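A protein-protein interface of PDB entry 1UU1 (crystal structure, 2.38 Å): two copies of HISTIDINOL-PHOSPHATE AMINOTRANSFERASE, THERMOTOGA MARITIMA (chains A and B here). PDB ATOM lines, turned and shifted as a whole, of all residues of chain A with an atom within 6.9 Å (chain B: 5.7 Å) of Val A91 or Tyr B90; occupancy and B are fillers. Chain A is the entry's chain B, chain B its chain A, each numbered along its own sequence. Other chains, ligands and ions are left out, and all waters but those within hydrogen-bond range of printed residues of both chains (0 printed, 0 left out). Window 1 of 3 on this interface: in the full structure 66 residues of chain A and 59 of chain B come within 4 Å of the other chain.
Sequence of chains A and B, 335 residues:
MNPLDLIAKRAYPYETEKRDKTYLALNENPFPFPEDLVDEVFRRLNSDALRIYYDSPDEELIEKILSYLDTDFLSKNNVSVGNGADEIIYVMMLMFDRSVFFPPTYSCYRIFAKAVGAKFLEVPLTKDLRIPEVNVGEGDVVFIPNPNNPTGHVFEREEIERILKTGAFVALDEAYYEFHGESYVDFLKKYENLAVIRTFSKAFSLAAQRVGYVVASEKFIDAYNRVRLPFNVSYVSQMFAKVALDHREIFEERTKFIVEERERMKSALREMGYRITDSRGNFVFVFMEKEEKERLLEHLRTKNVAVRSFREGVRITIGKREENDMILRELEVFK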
ATOM      1  N   ALA A  85       5.841  -6.210   0.745  1.00  0.00           N
ATOM      2  CA  ALA A  85       7.229  -5.745   0.843  1.00  0.00           C
ATOM      3  C   ALA A  85       7.344  -5.123   2.250  1.00  0.00           C
ATOM      4  O   ALA A  85       8.429  -5.004   2.807  1.00  0.00           O
ATOM      5  CB  ALA A  85       7.518  -4.709  -0.211  1.00  0.00           C
ATOM      6  N   ASP A  86       6.191  -4.731   2.790  1.00  0.00           N
ATOM      7  CA  ASP A  86       6.092  -4.172   4.124  1.00  0.00           C
ATOM      8  C   ASP A  86       6.773  -5.061   5.185  1.00  0.00           C
ATOM      9  O   ASP A  86       7.505  -4.574   6.043  1.00  0.00           O
ATOM     10  CB  ASP A  86       4.601  -3.972   4.508  1.00  0.00           C
ATOM     11  CG  ASP A  86       4.158  -2.511   4.395  1.00  0.00           C
ATOM     12  OD1 ASP A  86       4.914  -1.726   3.780  1.00  0.00           O
ATOM     13  OD2 ASP A  86       3.075  -2.140   4.910  1.00  0.00           O
ATOM     14  N   GLU A  87       6.522  -6.362   5.131  1.00  0.00           N
ATOM     15  CA  GLU A  87       7.108  -7.274   6.112  1.00  0.00           C
ATOM     16  C   GLU A  87       8.603  -7.404   5.936  1.00  0.00           C
ATOM     17  O   GLU A  87       9.338  -7.584   6.887  1.00  0.00           O
ATOM     18  CB  GLU A  87       6.489  -8.655   6.007  1.00  0.00           C
ATOM     19  CG  GLU A  87       7.042  -9.638   7.034  1.00  0.00           C
ATOM     20  CD  GLU A  87       6.421 -11.035   6.924  1.00  0.00           C
ATOM     21  OE1 GLU A  87       6.538 -11.650   5.844  1.00  0.00           O
ATOM     22  OE2 GLU A  87       5.822 -11.529   7.918  1.00  0.00           O
ATOM     23  N   ILE A  88       9.041  -7.362   4.693  1.00  0.00           N
ATOM     24  CA  ILE A  88      10.448  -7.462   4.386  1.00  0.00           C
ATOM     25  C   ILE A  88      11.217  -6.312   5.038  1.00  0.00           C
ATOM     26  O   ILE A  88      12.296  -6.498   5.606  1.00  0.00           O
ATOM     27  CB  ILE A  88      10.660  -7.404   2.870  1.00  0.00           C
ATOM     28  CG1 ILE A  88       9.842  -8.522   2.209  1.00  0.00           C
ATOM     29  CG2 ILE A  88      12.144  -7.526   2.541  1.00  0.00           C
ATOM     30  CD1 ILE A  88      10.051  -8.617   0.711  1.00  0.00           C
ATOM     31  N   ILE A  89      10.648  -5.117   4.932  1.00  0.00           N
ATOM     32  CA  ILE A  89      11.225  -3.908   5.510  1.00  0.00           C
ATOM     33  C   ILE A  89      11.175  -4.059   7.037  1.00  0.00           C
ATOM     34  O   ILE A  89      12.169  -3.838   7.750  1.00  0.00           O
ATOM     35  CB  ILE A  89      10.394  -2.647   5.087  1.00  0.00           C
ATOM     36  CG1 ILE A  89      10.670  -2.299   3.626  1.00  0.00           C
ATOM     37  CG2 ILE A  89      10.723  -1.467   5.974  1.00  0.00           C
ATOM     38  CD1 ILE A  89       9.720  -1.283   3.119  1.00  0.00           C
ATOM     39  N   TYR A  90      10.003  -4.447   7.520  1.00  0.00           N
ATOM     40  CA  TYR A  90       9.773  -4.634   8.931  1.00  0.00           C
ATOM     41  C   TYR A  90      10.766  -5.627   9.512  1.00  0.00           C
ATOM     42  O   TYR A  90      11.449  -5.312  10.479  1.00  0.00           O
ATOM     43  CB  TYR A  90       8.323  -5.105   9.162  1.00  0.00           C
ATOM     44  CG  TYR A  90       7.865  -5.152  10.608  1.00  0.00           C
ATOM     45  CD1 TYR A  90       8.104  -6.280  11.381  1.00  0.00           C
ATOM     46  CD2 TYR A  90       7.043  -4.154  11.132  1.00  0.00           C
ATOM     47  CE1 TYR A  90       7.518  -6.442  12.630  1.00  0.00           C
ATOM     48  CE2 TYR A  90       6.450  -4.304  12.379  1.00  0.00           C
ATOM     49  CZ  TYR A  90       6.689  -5.456  13.126  1.00  0.00           C
ATOM     50  OH  TYR A  90       6.091  -5.622  14.372  1.00  0.00           O
ATOM     51  N   VAL A  91      10.885  -6.812   8.926  1.00  0.00           N
ATOM     52  CA  VAL A  91      11.826  -7.754   9.507  1.00  0.00           C
ATOM     53  C   VAL A  91      13.249  -7.260   9.315  1.00  0.00           C
ATOM     54  O   VAL A  91      14.078  -7.412  10.196  1.00  0.00           O
ATOM     55  CB  VAL A  91      11.660  -9.217   8.957  1.00  0.00           C
ATOM     56  CG1 VAL A  91      10.180  -9.645   9.024  1.00  0.00           C
ATOM     57  CG2 VAL A  91      12.233  -9.338   7.589  1.00  0.00           C
ATOM     58  N   MET A  92      13.529  -6.625   8.183  1.00  0.00           N
ATOM     59  CA  MET A  92      14.864  -6.091   7.966  1.00  0.00           C
ATOM     60  C   MET A  92      15.275  -5.156   9.091  1.00  0.00           C
ATOM     61  O   MET A  92      16.466  -5.048   9.416  1.00  0.00           O
ATOM     62  CB  MET A  92      14.936  -5.332   6.644  1.00  0.00           C
ATOM     63  CG  MET A  92      15.413  -6.187   5.503  1.00  0.00           C
ATOM     64  SD  MET A  92      15.425  -5.403   3.896  1.00  0.00           S
ATOM     65  CE  MET A  92      17.146  -5.064   3.677  1.00  0.00           C
ATOM     66  N   MET A  93      14.300  -4.447   9.668  1.00  0.00           N
ATOM     67  CA  MET A  93      14.633  -3.551  10.783  1.00  0.00           C
ATOM     68  C   MET A  93      14.951  -4.318  12.074  1.00  0.00           C
ATOM     69  O   MET A  93      15.518  -3.771  13.025  1.00  0.00           O
ATOM     70  CB  MET A  93      13.505  -2.579  11.046  1.00  0.00           C
ATOM     71  CG  MET A  93      13.210  -1.685   9.874  1.00  0.00           C
ATOM     72  SD  MET A  93      11.972  -0.484  10.290  1.00  0.00           S
ATOM     73  CE  MET A  93      12.593   0.960   9.508  1.00  0.00           C
ATOM     74  N   LEU A  94      14.576  -5.588  12.109  1.00  0.00           N
ATOM     75  CA  LEU A  94      14.836  -6.420  13.272  1.00  0.00           C
ATOM     76  C   LEU A  94      16.248  -6.992  13.151  1.00  0.00           C
ATOM     77  O   LEU A  94      16.888  -7.339  14.139  1.00  0.00           O
ATOM     78  CB  LEU A  94      13.819  -7.559  13.326  1.00  0.00           C
ATOM     79  CG  LEU A  94      12.363  -7.130  13.544  1.00  0.00           C
ATOM     80  CD1 LEU A  94      11.448  -8.349  13.616  1.00  0.00           C
ATOM     81  CD2 LEU A  94      12.277  -6.347  14.831  1.00  0.00           C
ATOM     82  N   MET A  95      16.714  -7.072  11.913  1.00  0.00           N
ATOM     83  CA  MET A  95      18.006  -7.637  11.615  1.00  0.00           C
ATOM     84  C   MET A  95      19.205  -6.715  11.829  1.00  0.00           C
ATOM     85  O   MET A  95      20.244  -7.176  12.279  1.00  0.00           O
ATOM     86  CB  MET A  95      18.026  -8.116  10.173  1.00  0.00           C
ATOM     87  CG  MET A  95      16.936  -9.087   9.826  1.00  0.00           C
ATOM     88  SD  MET A  95      17.156  -9.687   8.145  1.00  0.00           S
ATOM     89  CE  MET A  95      16.048  -8.709   7.318  1.00  0.00           C
ATOM     90  N   PHE A  96      19.089  -5.432  11.506  1.00  0.00           N
ATOM     91  CA  PHE A  96      20.240  -4.563  11.660  1.00  0.00           C
ATOM     92  C   PHE A  96      20.263  -3.687  12.908  1.00  0.00           C
ATOM     93  O   PHE A  96      19.236  -3.474  13.561  1.00  0.00           O
ATOM     94  CB  PHE A  96      20.395  -3.720  10.410  1.00  0.00           C
ATOM     95  CG  PHE A  96      20.568  -4.530   9.149  1.00  0.00           C
ATOM     96  CD1 PHE A  96      21.832  -4.817   8.648  1.00  0.00           C
ATOM     97  CD2 PHE A  96      19.450  -4.985   8.443  1.00  0.00           C
ATOM     98  CE1 PHE A  96      21.980  -5.537   7.461  1.00  0.00           C
ATOM     99  CE2 PHE A  96      19.587  -5.705   7.254  1.00  0.00           C
ATOM    100  CZ  PHE A  96      20.848  -5.981   6.760  1.00  0.00           C
ATOM    101  N   PHE A 112       7.312   1.951  11.247  1.00  0.00           N
ATOM    102  CA  PHE A 112       7.743   0.608  11.617  1.00  0.00           C
ATOM    103  C   PHE A 112       8.937   0.647  12.544  1.00  0.00           C
ATOM    104  O   PHE A 112       9.039  -0.163  13.454  1.00  0.00           O
ATOM    105  CB  PHE A 112       8.080  -0.227  10.382  1.00  0.00           C
ATOM    106  CG  PHE A 112       6.904  -0.484   9.481  1.00  0.00           C
ATOM    107  CD1 PHE A 112       5.634  -0.016   9.800  1.00  0.00           C
ATOM    108  CD2 PHE A 112       7.071  -1.188   8.305  1.00  0.00           C
ATOM    109  CE1 PHE A 112       4.554  -0.247   8.949  1.00  0.00           C
ATOM    110  CE2 PHE A 112       6.003  -1.422   7.457  1.00  0.00           C
ATOM    111  CZ  PHE A 112       4.748  -0.956   7.768  1.00  0.00           C
ATOM    112  N   VAL A 116       8.664  -1.192  16.171  1.00  0.00           N
ATOM    113  CA  VAL A 116       9.505  -2.263  16.670  1.00  0.00           C
ATOM    114  C   VAL A 116      10.503  -1.743  17.708  1.00  0.00           C
ATOM    115  O   VAL A 116      11.260  -2.513  18.286  1.00  0.00           O
ATOM    116  CB  VAL A 116      10.258  -2.914  15.501  1.00  0.00           C
ATOM    117  CG1 VAL A 116      11.240  -3.906  16.022  1.00  0.00           C
ATOM    118  CG2 VAL A 116       9.265  -3.617  14.564  1.00  0.00           C
ATOM    119  N   PHE A 143      17.611   2.474   3.925  1.00  0.00           N
ATOM    120  CA  PHE A 143      16.414   2.265   3.135  1.00  0.00           C
ATOM    121  C   PHE A 143      16.258   3.313   2.070  1.00  0.00           C
ATOM    122  O   PHE A 143      16.053   4.487   2.365  1.00  0.00           O
ATOM    123  CB  PHE A 143      15.194   2.269   4.035  1.00  0.00           C
ATOM    124  CG  PHE A 143      15.045   1.026   4.833  1.00  0.00           C
ATOM    125  CD1 PHE A 143      14.599  -0.146   4.230  1.00  0.00           C
ATOM    126  CD2 PHE A 143      15.359   1.011   6.179  1.00  0.00           C
ATOM    127  CE1 PHE A 143      14.468  -1.325   4.968  1.00  0.00           C
ATOM    128  CE2 PHE A 143      15.234  -0.158   6.935  1.00  0.00           C
ATOM    129  CZ  PHE A 143      14.790  -1.327   6.338  1.00  0.00           C
ATOM    130  N   PHE A 220      22.434 -13.208   2.817  1.00  0.00           N
ATOM    131  CA  PHE A 220      21.385 -12.360   3.339  1.00  0.00           C
ATOM    132  C   PHE A 220      20.054 -13.129   3.349  1.00  0.00           C
ATOM    133  O   PHE A 220      19.389 -13.247   4.417  1.00  0.00           O
ATOM    134  CB  PHE A 220      21.210 -11.102   2.494  1.00  0.00           C
ATOM    135  CG  PHE A 220      20.034 -10.281   2.912  1.00  0.00           C
ATOM    136  CD1 PHE A 220      20.077  -9.504   4.082  1.00  0.00           C
ATOM    137  CD2 PHE A 220      18.845 -10.355   2.195  1.00  0.00           C
ATOM    138  CE1 PHE A 220      18.936  -8.818   4.530  1.00  0.00           C
ATOM    139  CE2 PHE A 220      17.701  -9.676   2.629  1.00  0.00           C
ATOM    140  CZ  PHE A 220      17.744  -8.912   3.790  1.00  0.00           C
ATOM    141  N   TYR A 224      17.673 -13.555   6.429  1.00  0.00           N
ATOM    142  CA  TYR A 224      16.289 -13.111   6.369  1.00  0.00           C
ATOM    143  C   TYR A 224      15.346 -14.277   6.689  1.00  0.00           C
ATOM    144  O   TYR A 224      14.435 -14.164   7.520  1.00  0.00           O
ATOM    145  CB  TYR A 224      16.028 -12.556   4.963  1.00  0.00           C
ATOM    146  CG  TYR A 224      14.595 -12.263   4.655  1.00  0.00           C
ATOM    147  CD1 TYR A 224      13.970 -11.140   5.177  1.00  0.00           C
ATOM    148  CD2 TYR A 224      13.833 -13.154   3.892  1.00  0.00           C
ATOM    149  CE1 TYR A 224      12.618 -10.915   4.960  1.00  0.00           C
ATOM    150  CE2 TYR A 224      12.479 -12.936   3.675  1.00  0.00           C
ATOM    151  CZ  TYR A 224      11.881 -11.817   4.215  1.00  0.00           C
ATOM    152  OH  TYR A 224      10.544 -11.579   4.028  1.00  0.00           O
ATOM    153  N   ARG A 226      15.719 -16.836   8.431  1.00  0.00           N
ATOM    154  CA  ARG A 226      15.768 -17.327   9.798  1.00  0.00           C
ATOM    155  C   ARG A 226      15.061 -16.337  10.708  1.00  0.00           C
ATOM    156  O   ARG A 226      14.662 -16.660  11.823  1.00  0.00           O
ATOM    157  CB  ARG A 226      17.219 -17.469  10.275  1.00  0.00           C
ATOM    158  CG  ARG A 226      18.140 -18.258   9.349  1.00  0.00           C
ATOM    159  CD  ARG A 226      19.433 -18.631  10.055  1.00  0.00           C
ATOM    160  NE  ARG A 226      20.401 -19.253   9.160  1.00  0.00           N
ATOM    161  CZ  ARG A 226      21.522 -19.841   9.572  1.00  0.00           C
ATOM    162  NH1 ARG A 226      22.352 -20.383   8.692  1.00  0.00           N
ATOM    163  NH2 ARG A 226      21.812 -19.899  10.868  1.00  0.00           N
ATOM    164  N   VAL A 227      14.889 -15.125  10.223  1.00  0.00           N
ATOM    165  CA  VAL A 227      14.273 -14.097  11.043  1.00  0.00           C
ATOM    166  C   VAL A 227      12.797 -13.834  10.774  1.00  0.00           C
ATOM    167  O   VAL A 227      12.048 -13.376  11.651  1.00  0.00           O
ATOM    168  CB  VAL A 227      15.080 -12.799  10.897  1.00  0.00           C
ATOM    169  CG1 VAL A 227      14.332 -11.625  11.524  1.00  0.00           C
ATOM    170  CG2 VAL A 227      16.424 -12.991  11.547  1.00  0.00           C
ATOM    171  N   ARG A 228      12.388 -14.117   9.549  1.00  0.00           N
ATOM    172  CA  ARG A 228      11.001 -13.934   9.157  1.00  0.00           C
ATOM    173  C   ARG A 228      10.102 -15.076   9.626  1.00  0.00           C
ATOM    174  O   ARG A 228      10.561 -16.181   9.915  1.00  0.00           O
ATOM    175  CB  ARG A 228      10.898 -13.868   7.646  1.00  0.00           C
ATOM    176  CG  ARG A 228      11.011 -15.229   6.965  1.00  0.00           C
ATOM    177  CD  ARG A 228      10.841 -15.084   5.438  1.00  0.00           C
ATOM    178  NE  ARG A 228      11.220 -16.278   4.689  1.00  0.00           N
ATOM    179  CZ  ARG A 228      10.463 -17.361   4.601  1.00  0.00           C
ATOM    180  NH1 ARG A 228       9.274 -17.395   5.206  1.00  0.00           N
ATOM    181  NH2 ARG A 228      10.900 -18.417   3.924  1.00  0.00           N
ATOM    182  N   LEU A 229       8.806 -14.808   9.670  1.00  0.00           N
ATOM    183  CA  LEU A 229       7.848 -15.847  10.031  1.00  0.00           C
ATOM    184  C   LEU A 229       7.976 -16.942   8.948  1.00  0.00           C
ATOM    185  O   LEU A 229       8.017 -16.647   7.747  1.00  0.00           O
ATOM    186  CB  LEU A 229       6.428 -15.261  10.079  1.00  0.00           C
ATOM    187  CG  LEU A 229       6.081 -14.476  11.359  1.00  0.00           C
ATOM    188  CD1 LEU A 229       5.053 -13.411  11.081  1.00  0.00           C
ATOM    189  CD2 LEU A 229       5.566 -15.445  12.399  1.00  0.00           C
ATOM    190  N   PRO A 230       8.072 -18.208   9.368  1.00  0.00           N
ATOM    191  CA  PRO A 230       8.206 -19.356   8.455  1.00  0.00           C
ATOM    192  C   PRO A 230       7.123 -19.395   7.377  1.00  0.00           C
ATOM    193  O   PRO A 230       7.405 -19.588   6.187  1.00  0.00           O
ATOM    194  CB  PRO A 230       8.092 -20.562   9.389  1.00  0.00           C
ATOM    195  CG  PRO A 230       8.473 -20.024  10.721  1.00  0.00           C
ATOM    196  CD  PRO A 230       7.894 -18.657  10.759  1.00  0.00           C
ATOM    197  N   ALA B  85      -1.461 -17.478  14.111  1.00  0.00           N
ATOM    198  CA  ALA B  85      -1.355 -17.210  15.544  1.00  0.00           C
ATOM    199  C   ALA B  85       0.123 -16.858  15.753  1.00  0.00           C
ATOM    200  O   ALA B  85       0.476 -16.099  16.651  1.00  0.00           O
ATOM    201  CB  ALA B  85      -1.718 -18.452  16.351  1.00  0.00           C
ATOM    202  N   ASP B  86       0.969 -17.439  14.905  1.00  0.00           N
ATOM    203  CA  ASP B  86       2.410 -17.192  14.891  1.00  0.00           C
ATOM    204  C   ASP B  86       2.722 -15.702  14.900  1.00  0.00           C
ATOM    205  O   ASP B  86       3.554 -15.264  15.681  1.00  0.00           O
ATOM    206  CB  ASP B  86       3.048 -17.784  13.638  1.00  0.00           C
ATOM    207  CG  ASP B  86       3.441 -19.245  13.793  1.00  0.00           C
ATOM    208  OD1 ASP B  86       3.938 -19.798  12.788  1.00  0.00           O
ATOM    209  OD2 ASP B  86       3.277 -19.842  14.881  1.00  0.00           O
ATOM    210  N   GLU B  87       2.062 -14.914  14.047  1.00  0.00           N
ATOM    211  CA  GLU B  87       2.359 -13.477  14.028  1.00  0.00           C
ATOM    212  C   GLU B  87       2.021 -12.795  15.336  1.00  0.00           C
ATOM    213  O   GLU B  87       2.720 -11.884  15.784  1.00  0.00           O
ATOM    214  CB  GLU B  87       1.635 -12.751  12.896  1.00  0.00           C
ATOM    215  CG  GLU B  87       2.284 -11.365  12.601  1.00  0.00           C
ATOM    216  CD  GLU B  87       1.417 -10.451  11.747  1.00  0.00           C
ATOM    217  OE1 GLU B  87       0.190 -10.510  11.914  1.00  0.00           O
ATOM    218  OE2 GLU B  87       1.949  -9.664  10.923  1.00  0.00           O
ATOM    219  N   ILE B  88       0.963 -13.259  15.978  1.00  0.00           N
ATOM    220  CA  ILE B  88       0.552 -12.655  17.223  1.00  0.00           C
ATOM    221  C   ILE B  88       1.606 -12.936  18.260  1.00  0.00           C
ATOM    222  O   ILE B  88       1.863 -12.116  19.120  1.00  0.00           O
ATOM    223  CB  ILE B  88      -0.802 -13.214  17.677  1.00  0.00           C
ATOM    224  CG1 ILE B  88      -1.836 -12.976  16.571  1.00  0.00           C
ATOM    225  CG2 ILE B  88      -1.223 -12.566  19.001  1.00  0.00           C
ATOM    226  CD1 ILE B  88      -3.205 -13.646  16.808  1.00  0.00           C
ATOM    227  N   ILE B  89       2.243 -14.090  18.153  1.00  0.00           N
ATOM    228  CA  ILE B  89       3.263 -14.461  19.117  1.00  0.00           C
ATOM    229  C   ILE B  89       4.493 -13.609  18.854  1.00  0.00           C
ATOM    230  O   ILE B  89       5.090 -13.032  19.768  1.00  0.00           O
ATOM    231  CB  ILE B  89       3.586 -15.936  18.964  1.00  0.00           C
ATOM    232  CG1 ILE B  89       2.387 -16.760  19.445  1.00  0.00           C
ATOM    233  CG2 ILE B  89       4.856 -16.283  19.707  1.00  0.00           C
ATOM    234  CD1 ILE B  89       2.471 -18.251  19.093  1.00  0.00           C
ATOM    235  N   TYR B  90       4.836 -13.530  17.576  1.00  0.00           N
ATOM    236  CA  TYR B  90       5.985 -12.781  17.100  1.00  0.00           C
ATOM    237  C   TYR B  90       5.959 -11.301  17.521  1.00  0.00           C
ATOM    238  O   TYR B  90       6.948 -10.762  18.016  1.00  0.00           O
ATOM    239  CB  TYR B  90       6.011 -12.907  15.576  1.00  0.00           C
ATOM    240  CG  TYR B  90       7.293 -12.510  14.890  1.00  0.00           C
ATOM    241  CD1 TYR B  90       7.550 -11.179  14.553  1.00  0.00           C
ATOM    242  CD2 TYR B  90       8.156 -13.489  14.403  1.00  0.00           C
ATOM    243  CE1 TYR B  90       8.634 -10.846  13.722  1.00  0.00           C
ATOM    244  CE2 TYR B  90       9.222 -13.173  13.575  1.00  0.00           C
ATOM    245  CZ  TYR B  90       9.454 -11.862  13.238  1.00  0.00           C
ATOM    246  OH  TYR B  90      10.506 -11.594  12.403  1.00  0.00           O
ATOM    247  N   VAL B  91       4.816 -10.646  17.325  1.00  0.00           N
ATOM    248  CA  VAL B  91       4.694  -9.248  17.671  1.00  0.00           C
ATOM    249  C   VAL B  91       4.706  -9.050  19.179  1.00  0.00           C
ATOM    250  O   VAL B  91       5.337  -8.130  19.679  1.00  0.00           O
ATOM    251  CB  VAL B  91       3.427  -8.642  17.068  1.00  0.00           C
ATOM    252  CG1 VAL B  91       3.556  -8.577  15.539  1.00  0.00           C
ATOM    253  CG2 VAL B  91       2.253  -9.491  17.444  1.00  0.00           C
ATOM    254  N   MET B  92       4.025  -9.928  19.905  1.00  0.00           N
ATOM    255  CA  MET B  92       3.994  -9.819  21.352  1.00  0.00           C
ATOM    256  C   MET B  92       5.418  -9.815  21.888  1.00  0.00           C
ATOM    257  O   MET B  92       5.754  -9.048  22.805  1.00  0.00           O
ATOM    258  CB  MET B  92       3.175 -10.959  21.964  1.00  0.00           C
ATOM    259  CG  MET B  92       1.703 -10.789  21.662  1.00  0.00           C
ATOM    260  SD  MET B  92       0.561 -11.923  22.442  1.00  0.00           S
ATOM    261  CE  MET B  92       0.490 -11.257  24.087  1.00  0.00           C
ATOM    262  N   MET B  93       6.271 -10.644  21.302  1.00  0.00           N
ATOM    263  CA  MET B  93       7.644 -10.680  21.763  1.00  0.00           C
ATOM    264  C   MET B  93       8.370  -9.370  21.501  1.00  0.00           C
ATOM    265  O   MET B  93       9.422  -9.113  22.097  1.00  0.00           O
ATOM    266  CB  MET B  93       8.389 -11.840  21.121  1.00  0.00           C
ATOM    267  CG  MET B  93       7.935 -13.177  21.664  1.00  0.00           C
ATOM    268  SD  MET B  93       8.819 -14.597  21.026  1.00  0.00           S
ATOM    269  CE  MET B  93       7.954 -15.908  21.924  1.00  0.00           C
ATOM    270  N   LEU B  94       7.819  -8.537  20.620  1.00  0.00           N
ATOM    271  CA  LEU B  94       8.440  -7.246  20.354  1.00  0.00           C
ATOM    272  C   LEU B  94       7.883  -6.215  21.332  1.00  0.00           C
ATOM    273  O   LEU B  94       8.477  -5.165  21.534  1.00  0.00           O
ATOM    274  CB  LEU B  94       8.183  -6.777  18.908  1.00  0.00           C
ATOM    275  CG  LEU B  94       8.864  -7.545  17.762  1.00  0.00           C
ATOM    276  CD1 LEU B  94       8.442  -6.951  16.443  1.00  0.00           C
ATOM    277  CD2 LEU B  94      10.360  -7.483  17.903  1.00  0.00           C
ATOM    278  N   PHE B 112      11.055 -17.733  17.446  1.00  0.00           N
ATOM    279  CA  PHE B 112      10.666 -16.349  17.215  1.00  0.00           C
ATOM    280  C   PHE B 112      11.384 -15.371  18.154  1.00  0.00           C
ATOM    281  O   PHE B 112      11.650 -14.228  17.774  1.00  0.00           O
ATOM    282  CB  PHE B 112       9.140 -16.176  17.365  1.00  0.00           C
ATOM    283  CG  PHE B 112       8.319 -16.991  16.382  1.00  0.00           C
ATOM    284  CD1 PHE B 112       8.927 -17.666  15.302  1.00  0.00           C
ATOM    285  CD2 PHE B 112       6.928 -17.108  16.559  1.00  0.00           C
ATOM    286  CE1 PHE B 112       8.157 -18.457  14.408  1.00  0.00           C
ATOM    287  CE2 PHE B 112       6.117 -17.905  15.667  1.00  0.00           C
ATOM    288  CZ  PHE B 112       6.734 -18.576  14.596  1.00  0.00           C
ATOM    289  N   ALA B 115      14.903 -15.061  16.913  1.00  0.00           N
ATOM    290  CA  ALA B 115      14.703 -14.351  15.658  1.00  0.00           C
ATOM    291  C   ALA B 115      14.358 -12.885  15.822  1.00  0.00           C
ATOM    292  O   ALA B 115      14.841 -12.045  15.079  1.00  0.00           O
ATOM    293  CB  ALA B 115      13.613 -15.048  14.833  1.00  0.00           C
ATOM    294  N   VAL B 116      13.520 -12.579  16.797  1.00  0.00           N
ATOM    295  CA  VAL B 116      13.100 -11.207  17.030  1.00  0.00           C
ATOM    296  C   VAL B 116      14.010 -10.467  18.012  1.00  0.00           C
ATOM    297  O   VAL B 116      13.775  -9.303  18.328  1.00  0.00           O
ATOM    298  CB  VAL B 116      11.633 -11.185  17.517  1.00  0.00           C
ATOM    299  CG1 VAL B 116      11.525 -10.677  18.956  1.00  0.00           C
ATOM    300  CG2 VAL B 116      10.809 -10.360  16.565  1.00  0.00           C
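CG1 of Val A91 touches OH of Tyr B90 (3.9 Å).
Leu A94 touches Tyr B90.
Val B116 touches Leu A94.
CG2 of Val A116 touches CD1 of Leu B94 (3.9 Å).
CB of Ala B115 touches O of Arg A226, 3.6 Å away.
Ala B115 touches Val A227 (O to CG1, 3.6 Å).
Asp B86 touches Leu A229 (CB to CD2, 3.7 Å).
Glu B87 touches Leu A229.
Leu A229 touches Tyr B90.
Phe B112 touches Leu A229 (CZ to CD2, 3.999 Å).
Tyr A90 touches Leu B94, and with the chains exchanged Leu A94 touches Tyr B90.
Val A91 touches Tyr B90, but with the chains exchanged Tyr A90 does not touch Val B91 (4.1 Å).
Leu B94 touches its own counterpart, Leu A94.
Leu A94 touches Val B116, and with the chains exchanged Val A116 touches Leu B94.
Positions printed for both chains: 85, 86, 87, 88, 89, 90, 91, 92, 93, 94, 112 and 116.
The guanidinium group of Arg A228 is in hydrogen-bond range of the backbone carbonyl oxygen of Pro A230, 3.0 Å away.
Of the printed residues of chain B, Tyr A90 touches Leu B94 (3.4 Å).
Val A91 touches just one residue of chain B: Tyr B90.
Of the printed residues of chain B, Val A227 touches Tyr B90 (2.5 Å) and Ala B115 (3.6 Å).
Printed residues of chain B within 4 Å of Leu A229: Asp B86 (3.7 Å), Glu B87 (3.8 Å), Tyr B90 (3.8 Å) and Phe B112 (3.999 Å).
Tyr B90 touches four residues of chain A.
The nearest printed residue of chain B that does not touch Val A91 is Ala B115 (6.8 Å).
Hydrophobic or aromatic side chains of chain A that line the printed part of chain B: Tyr A90, Val A91, Leu A94, Val A116, Val A227, Leu A229 and Pro A230.
Of the 13 printed residues of chain B, 7 touch a printed residue of chain A.
Printed residues of chain B that touch a printed residue of chain A: Asp B86, Glu B87, Tyr B90, Leu B94, Phe B112, Ala B115 and Val B116.
OH of Tyr B90 sits at hydrogen-bond distance from O of Val A227, at 2.5 Å.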
